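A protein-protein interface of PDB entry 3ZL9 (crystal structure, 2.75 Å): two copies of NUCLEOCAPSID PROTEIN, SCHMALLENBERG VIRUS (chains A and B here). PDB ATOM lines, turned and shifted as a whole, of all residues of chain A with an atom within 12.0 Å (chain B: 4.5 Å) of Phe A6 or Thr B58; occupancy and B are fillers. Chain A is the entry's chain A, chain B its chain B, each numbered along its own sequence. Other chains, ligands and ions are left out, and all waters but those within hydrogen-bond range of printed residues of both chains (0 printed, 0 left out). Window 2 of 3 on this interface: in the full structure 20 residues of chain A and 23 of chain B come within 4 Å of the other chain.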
ATOM      1  N   SER A   4     -24.147  -7.092  -1.463  1.00  0.00           N
ATOM      2  CA  SER A   4     -23.831  -7.322   0.003  1.00  0.00           C
ATOM      3  C   SER A   4     -22.493  -6.660   0.497  1.00  0.00           C
ATOM      4  O   SER A   4     -22.359  -5.424   0.494  1.00  0.00           O
ATOM      5  CB  SER A   4     -23.868  -8.839   0.316  1.00  0.00           C
ATOM      6  OG  SER A   4     -24.184  -9.100   1.667  1.00  0.00           O
ATOM      7  N   GLN A   5     -21.527  -7.460   0.953  1.00  0.00           N
ATOM      8  CA  GLN A   5     -20.292  -6.928   1.491  1.00  0.00           C
ATOM      9  C   GLN A   5     -20.656  -5.943   2.586  1.00  0.00           C
ATOM     10  O   GLN A   5     -20.348  -4.734   2.557  1.00  0.00           O
ATOM     11  CB  GLN A   5     -19.360  -6.291   0.464  1.00  0.00           C
ATOM     12  CG  GLN A   5     -18.417  -7.260  -0.228  1.00  0.00           C
ATOM     13  CD  GLN A   5     -17.556  -6.581  -1.290  1.00  0.00           C
ATOM     14  OE1 GLN A   5     -17.986  -5.616  -1.943  1.00  0.00           O
ATOM     15  NE2 GLN A   5     -16.331  -7.081  -1.464  1.00  0.00           N
ATOM     16  N   PHE A   6     -21.388  -6.512   3.528  1.00  0.00           N
ATOM     17  CA  PHE A   6     -21.316  -6.081   4.895  1.00  0.00           C
ATOM     18  C   PHE A   6     -20.196  -6.909   5.513  1.00  0.00           C
ATOM     19  O   PHE A   6     -20.165  -7.100   6.726  1.00  0.00           O
ATOM     20  CB  PHE A   6     -22.609  -6.340   5.632  1.00  0.00           C
ATOM     21  CG  PHE A   6     -23.766  -5.496   5.161  1.00  0.00           C
ATOM     22  CD1 PHE A   6     -23.595  -4.159   4.798  1.00  0.00           C
ATOM     23  CD2 PHE A   6     -25.047  -6.031   5.112  1.00  0.00           C
ATOM     24  CE1 PHE A   6     -24.671  -3.393   4.361  1.00  0.00           C
ATOM     25  CE2 PHE A   6     -26.119  -5.270   4.681  1.00  0.00           C
ATOM     26  CZ  PHE A   6     -25.932  -3.954   4.300  1.00  0.00           C
ATOM     27  N   ILE A   7     -19.294  -7.406   4.675  1.00  0.00           N
ATOM     28  CA  ILE A   7     -18.211  -8.231   5.138  1.00  0.00           C
ATOM     29  C   ILE A   7     -16.914  -7.665   4.579  1.00  0.00           C
ATOM     30  O   ILE A   7     -16.800  -7.423   3.383  1.00  0.00           O
ATOM     31  CB  ILE A   7     -18.412  -9.702   4.730  1.00  0.00           C
ATOM     32  CG1 ILE A   7     -19.688 -10.247   5.388  1.00  0.00           C
ATOM     33  CG2 ILE A   7     -17.199 -10.532   5.127  1.00  0.00           C
ATOM     34  CD1 ILE A   7     -20.122 -11.608   4.894  1.00  0.00           C
ATOM     35  N   PHE A   8     -15.949  -7.436   5.466  1.00  0.00           N
ATOM     36  CA  PHE A   8     -14.669  -6.879   5.082  1.00  0.00           C
ATOM     37  C   PHE A   8     -13.547  -7.784   5.558  1.00  0.00           C
ATOM     38  O   PHE A   8     -13.641  -8.376   6.644  1.00  0.00           O
ATOM     39  CB  PHE A   8     -14.490  -5.514   5.721  1.00  0.00           C
ATOM     40  CG  PHE A   8     -15.604  -4.563   5.450  1.00  0.00           C
ATOM     41  CD1 PHE A   8     -16.755  -4.586   6.223  1.00  0.00           C
ATOM     42  CD2 PHE A   8     -15.491  -3.613   4.459  1.00  0.00           C
ATOM     43  CE1 PHE A   8     -17.781  -3.679   6.002  1.00  0.00           C
ATOM     44  CE2 PHE A   8     -16.514  -2.690   4.240  1.00  0.00           C
ATOM     45  CZ  PHE A   8     -17.656  -2.725   5.011  1.00  0.00           C
ATOM     46  N   GLU A   9     -12.495  -7.901   4.746  1.00  0.00           N
ATOM     47  CA  GLU A   9     -11.321  -8.691   5.125  1.00  0.00           C
ATOM     48  C   GLU A   9     -10.011  -8.077   4.641  1.00  0.00           C
ATOM     49  O   GLU A   9     -10.012  -7.097   3.900  1.00  0.00           O
ATOM     50  CB  GLU A   9     -11.465 -10.139   4.635  1.00  0.00           C
ATOM     51  CG  GLU A   9     -11.343 -10.382   3.110  1.00  0.00           C
ATOM     52  CD  GLU A   9     -12.468  -9.782   2.289  1.00  0.00           C
ATOM     53  OE1 GLU A   9     -12.656  -8.539   2.279  1.00  0.00           O
ATOM     54  OE2 GLU A   9     -13.169 -10.564   1.616  1.00  0.00           O
ATOM     55  N   ASP A  10      -8.913  -8.685   5.085  1.00  0.00           N
ATOM     56  CA  ASP A  10      -7.571  -8.129   5.019  1.00  0.00           C
ATOM     57  C   ASP A  10      -7.046  -8.033   3.612  1.00  0.00           C
ATOM     58  O   ASP A  10      -7.262  -8.919   2.781  1.00  0.00           O
ATOM     59  CB  ASP A  10      -6.621  -9.003   5.868  1.00  0.00           C
ATOM     60  CG  ASP A  10      -5.306  -8.307   6.178  1.00  0.00           C
ATOM     61  OD1 ASP A  10      -5.435  -7.114   6.403  1.00  0.00           O
ATOM     62  OD2 ASP A  10      -4.172  -8.879   6.206  1.00  0.00           O
ATOM     63  N   VAL B  54     -21.244   2.609   3.403  1.00  0.00           N
ATOM     64  CA  VAL B  54     -22.312   1.639   3.167  1.00  0.00           C
ATOM     65  C   VAL B  54     -23.428   1.845   4.176  1.00  0.00           C
ATOM     66  O   VAL B  54     -24.596   1.707   3.833  1.00  0.00           O
ATOM     67  CB  VAL B  54     -21.840   0.166   3.120  1.00  0.00           C
ATOM     68  CG1 VAL B  54     -20.595   0.026   2.256  1.00  0.00           C
ATOM     69  CG2 VAL B  54     -21.607  -0.403   4.497  1.00  0.00           C
ATOM     70  N   LEU B  55     -23.071   2.210   5.405  1.00  0.00           N
ATOM     71  CA  LEU B  55     -24.073   2.600   6.387  1.00  0.00           C
ATOM     72  C   LEU B  55     -24.902   3.780   5.875  1.00  0.00           C
ATOM     73  O   LEU B  55     -26.130   3.790   6.013  1.00  0.00           O
ATOM     74  CB  LEU B  55     -23.437   2.926   7.744  1.00  0.00           C
ATOM     75  CG  LEU B  55     -22.937   1.734   8.571  1.00  0.00           C
ATOM     76  CD1 LEU B  55     -22.572   2.187   9.963  1.00  0.00           C
ATOM     77  CD2 LEU B  55     -23.937   0.597   8.689  1.00  0.00           C
ATOM     78  N   HIS B  56     -24.237   4.752   5.256  1.00  0.00           N
ATOM     79  CA  HIS B  56     -24.909   5.933   4.712  1.00  0.00           C
ATOM     80  C   HIS B  56     -25.936   5.559   3.648  1.00  0.00           C
ATOM     81  O   HIS B  56     -27.011   6.154   3.580  1.00  0.00           O
ATOM     82  CB  HIS B  56     -23.878   6.892   4.115  1.00  0.00           C
ATOM     83  CG  HIS B  56     -24.419   8.253   3.823  1.00  0.00           C
ATOM     84  ND1 HIS B  56     -24.964   8.592   2.602  1.00  0.00           N
ATOM     85  CD2 HIS B  56     -24.506   9.362   4.595  1.00  0.00           C
ATOM     86  CE1 HIS B  56     -25.361   9.852   2.632  1.00  0.00           C
ATOM     87  NE2 HIS B  56     -25.097  10.340   3.830  1.00  0.00           N
ATOM     88  N   LYS B  57     -25.591   4.581   2.813  1.00  0.00           N
ATOM     89  CA  LYS B  57     -26.438   4.136   1.703  1.00  0.00           C
ATOM     90  C   LYS B  57     -27.515   3.162   2.136  1.00  0.00           C
ATOM     91  O   LYS B  57     -28.414   2.880   1.351  1.00  0.00           O
ATOM     92  CB  LYS B  57     -25.613   3.393   0.657  1.00  0.00           C
ATOM     93  CG  LYS B  57     -24.519   4.196  -0.022  1.00  0.00           C
ATOM     94  CD  LYS B  57     -23.345   3.306  -0.434  1.00  0.00           C
ATOM     95  CE  LYS B  57     -23.734   2.115  -1.311  1.00  0.00           C
ATOM     96  NZ  LYS B  57     -24.032   2.520  -2.710  1.00  0.00           N
ATOM     97  N   THR B  58     -27.410   2.608   3.345  1.00  0.00           N
ATOM     98  CA  THR B  58     -28.249   1.481   3.726  1.00  0.00           C
ATOM     99  C   THR B  58     -29.358   1.899   4.706  1.00  0.00           C
ATOM    100  O   THR B  58     -29.097   2.458   5.758  1.00  0.00           O
ATOM    101  CB  THR B  58     -27.400   0.284   4.241  1.00  0.00           C
ATOM    102  OG1 THR B  58     -28.220  -0.872   4.425  1.00  0.00           O
ATOM    103  CG2 THR B  58     -26.744   0.585   5.536  1.00  0.00           C
ATOM    104  N   ALA B  59     -30.602   1.587   4.341  1.00  0.00           N
ATOM    105  CA  ALA B  59     -31.795   2.020   5.080  1.00  0.00           C
ATOM    106  C   ALA B  59     -32.251   0.969   6.092  1.00  0.00           C
ATOM    107  O   ALA B  59     -33.272   0.309   5.908  1.00  0.00           O
ATOM    108  CB  ALA B  59     -32.921   2.332   4.105  1.00  0.00           C
ATOM    109  N   GLN B  60     -31.491   0.824   7.163  1.00  0.00           N
ATOM    110  CA  GLN B  60     -31.713  -0.231   8.131  1.00  0.00           C
ATOM    111  C   GLN B  60     -31.030   0.206   9.422  1.00  0.00           C
ATOM    112  O   GLN B  60     -29.799   0.310   9.464  1.00  0.00           O
ATOM    113  CB  GLN B  60     -31.124  -1.530   7.592  1.00  0.00           C
ATOM    114  CG  GLN B  60     -31.500  -2.784   8.358  1.00  0.00           C
ATOM    115  CD  GLN B  60     -30.685  -3.985   7.901  1.00  0.00           C
ATOM    116  OE1 GLN B  60     -30.561  -4.242   6.704  1.00  0.00           O
ATOM    117  NE2 GLN B  60     -30.104  -4.715   8.853  1.00  0.00           N
ATOM    118  N   VAL B  63     -27.339  -2.666  11.751  1.00  0.00           N
ATOM    119  CA  VAL B  63     -26.839  -3.640  10.773  1.00  0.00           C
ATOM    120  C   VAL B  63     -25.679  -4.502  11.293  1.00  0.00           C
ATOM    121  O   VAL B  63     -24.930  -4.088  12.183  1.00  0.00           O
ATOM    122  CB  VAL B  63     -26.435  -2.980   9.426  1.00  0.00           C
ATOM    123  CG1 VAL B  63     -27.310  -1.774   9.103  1.00  0.00           C
ATOM    124  CG2 VAL B  63     -24.982  -2.579   9.414  1.00  0.00           C
ATOM    125  N   ASP B  64     -25.546  -5.699  10.718  1.00  0.00           N
ATOM    126  CA  ASP B  64     -24.525  -6.661  11.140  1.00  0.00           C
ATOM    127  C   ASP B  64     -23.328  -6.589  10.199  1.00  0.00           C
ATOM    128  O   ASP B  64     -23.401  -7.021   9.054  1.00  0.00           O
ATOM    129  CB  ASP B  64     -25.093  -8.085  11.168  1.00  0.00           C
ATOM    130  CG  ASP B  64     -26.015  -8.338  12.371  1.00  0.00           C
ATOM    131  OD1 ASP B  64     -26.369  -7.385  13.112  1.00  0.00           O
ATOM    132  OD2 ASP B  64     -26.360  -9.517  12.590  1.00  0.00           O
ATOM    133  N   LEU B  65     -22.237  -6.019  10.708  1.00  0.00           N
ATOM    134  CA  LEU B  65     -20.987  -5.844   9.960  1.00  0.00           C
ATOM    135  C   LEU B  65     -19.914  -6.799  10.468  1.00  0.00           C
ATOM    136  O   LEU B  65     -19.813  -7.056  11.675  1.00  0.00           O
ATOM    137  CB  LEU B  65     -20.470  -4.412  10.123  1.00  0.00           C
ATOM    138  CG  LEU B  65     -21.313  -3.324   9.460  1.00  0.00           C
ATOM    139  CD1 LEU B  65     -20.775  -1.956   9.811  1.00  0.00           C
ATOM    140  CD2 LEU B  65     -21.337  -3.520   7.951  1.00  0.00           C
ATOM    141  N   THR B  66     -19.081  -7.279   9.554  1.00  0.00           N
ATOM    142  CA  THR B  66     -18.129  -8.328   9.867  1.00  0.00           C
ATOM    143  C   THR B  66     -16.725  -7.906   9.447  1.00  0.00           C
ATOM    144  O   THR B  66     -16.461  -7.669   8.253  1.00  0.00           O
ATOM    145  CB  THR B  66     -18.564  -9.641   9.192  1.00  0.00           C
ATOM    146  OG1 THR B  66     -19.921  -9.935   9.573  1.00  0.00           O
ATOM    147  CG2 THR B  66     -17.640 -10.813   9.588  1.00  0.00           C
ATOM    148  N   ASN B  76     -26.863   1.828  12.937  1.00  0.00           N
ATOM    149  CA  ASN B  76     -26.682   2.690  11.777  1.00  0.00           C
ATOM    150  C   ASN B  76     -27.016   4.146  12.129  1.00  0.00           C
ATOM    151  O   ASN B  76     -28.177   4.576  12.145  1.00  0.00           O
ATOM    152  CB  ASN B  76     -27.501   2.237  10.582  1.00  0.00           C
ATOM    153  CG  ASN B  76     -27.169   3.022   9.323  1.00  0.00           C
ATOM    154  OD1 ASN B  76     -26.525   4.069   9.379  1.00  0.00           O
ATOM    155  ND2 ASN B  76     -27.623   2.527   8.180  1.00  0.00           N
ATOM    156  N   PHE B  79     -27.038   6.662   7.869  1.00  0.00           N
ATOM    157  CA  PHE B  79     -28.122   6.816   6.929  1.00  0.00           C
ATOM    158  C   PHE B  79     -28.776   8.165   7.245  1.00  0.00           C
ATOM    159  O   PHE B  79     -29.042   8.452   8.412  1.00  0.00           O
ATOM    160  CB  PHE B  79     -29.110   5.661   7.075  1.00  0.00           C
ATOM    161  CG  PHE B  79     -30.216   5.677   6.062  1.00  0.00           C
ATOM    162  CD1 PHE B  79     -29.965   5.372   4.730  1.00  0.00           C
ATOM    163  CD2 PHE B  79     -31.510   5.987   6.442  1.00  0.00           C
ATOM    164  CE1 PHE B  79     -30.985   5.384   3.797  1.00  0.00           C
ATOM    165  CE2 PHE B  79     -32.533   5.998   5.512  1.00  0.00           C
ATOM    166  CZ  PHE B  79     -32.270   5.696   4.191  1.00  0.00           C
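Phe A6 touches four residues of chain B.
Of the printed residues of chain B, Ile A7 touches Thr B66 (3.6 Å).
Of the printed residues of chain B, Phe A8 touches Thr B66 (2.8 Å).
Glu A9 touches none of the printed residues of chain B.
No residue of chain A comes within 4 Å of Val B54.
No residue of chain A comes within 4 Å of Lys B57.
Printed residues of chain A within 4 Å of Thr B58: Phe A6.
No residue of chain A comes within 4 Å of Gln B60.
No residue of chain A comes within 4 Å of Val B63.
Printed residues of chain A within 4 Å of Asp B64: Phe A6 (3.6 Å).
Of chain A, only Phe A6 comes within 4 Å of Leu B65.
No residue of chain A comes within 4 Å of Asn B76.
The nearest residue of chain B that does not touch Phe A6 is Val B54 (4.3 Å).
The nearest printed residue of chain A that does not touch Asp B64 is Ile A7 (6.0 Å).
No position is printed for both chains.
Of the 6 pairs that touch across the chains among the printed residues, none has its exchanged pair printed and touching as well.
OG1 of Thr B58 touches CZ of Phe A6, 3.8 Å away.
CB of Phe A6 touches O of Asp B64 (3.6 Å).
CA of Leu B65 touches O of Phe A6, at 3.6 Å.
O of Thr B66 touches CA of Ile A7 (3.6 Å).
The backbone carbonyl oxygen (O) of Thr B58 sits at hydrogen-bond distance from the side-chain amide nitrogen (ND2) of Asn B76 (2.8 Å).
Of the 7 printed residues of chain A, 3 touch a printed residue of chain B.
Of the 13 printed residues of chain B, 4 touch a printed residue of chain A.
Hydrophobic or aromatic side chains of chain B that line the printed part of chain A: Leu B65.
Among the printed residues, 6 pairs touch across the chains.
The backbone carbonyl oxygen (O) of Phe A6 is in hydrogen-bond range of the backbone NH (N) of Thr B66, at 3.0 Å.
The backbone NH of Phe A8 lies within hydrogen-bond range of the backbone carbonyl oxygen of Thr B66 (2.8 Å).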
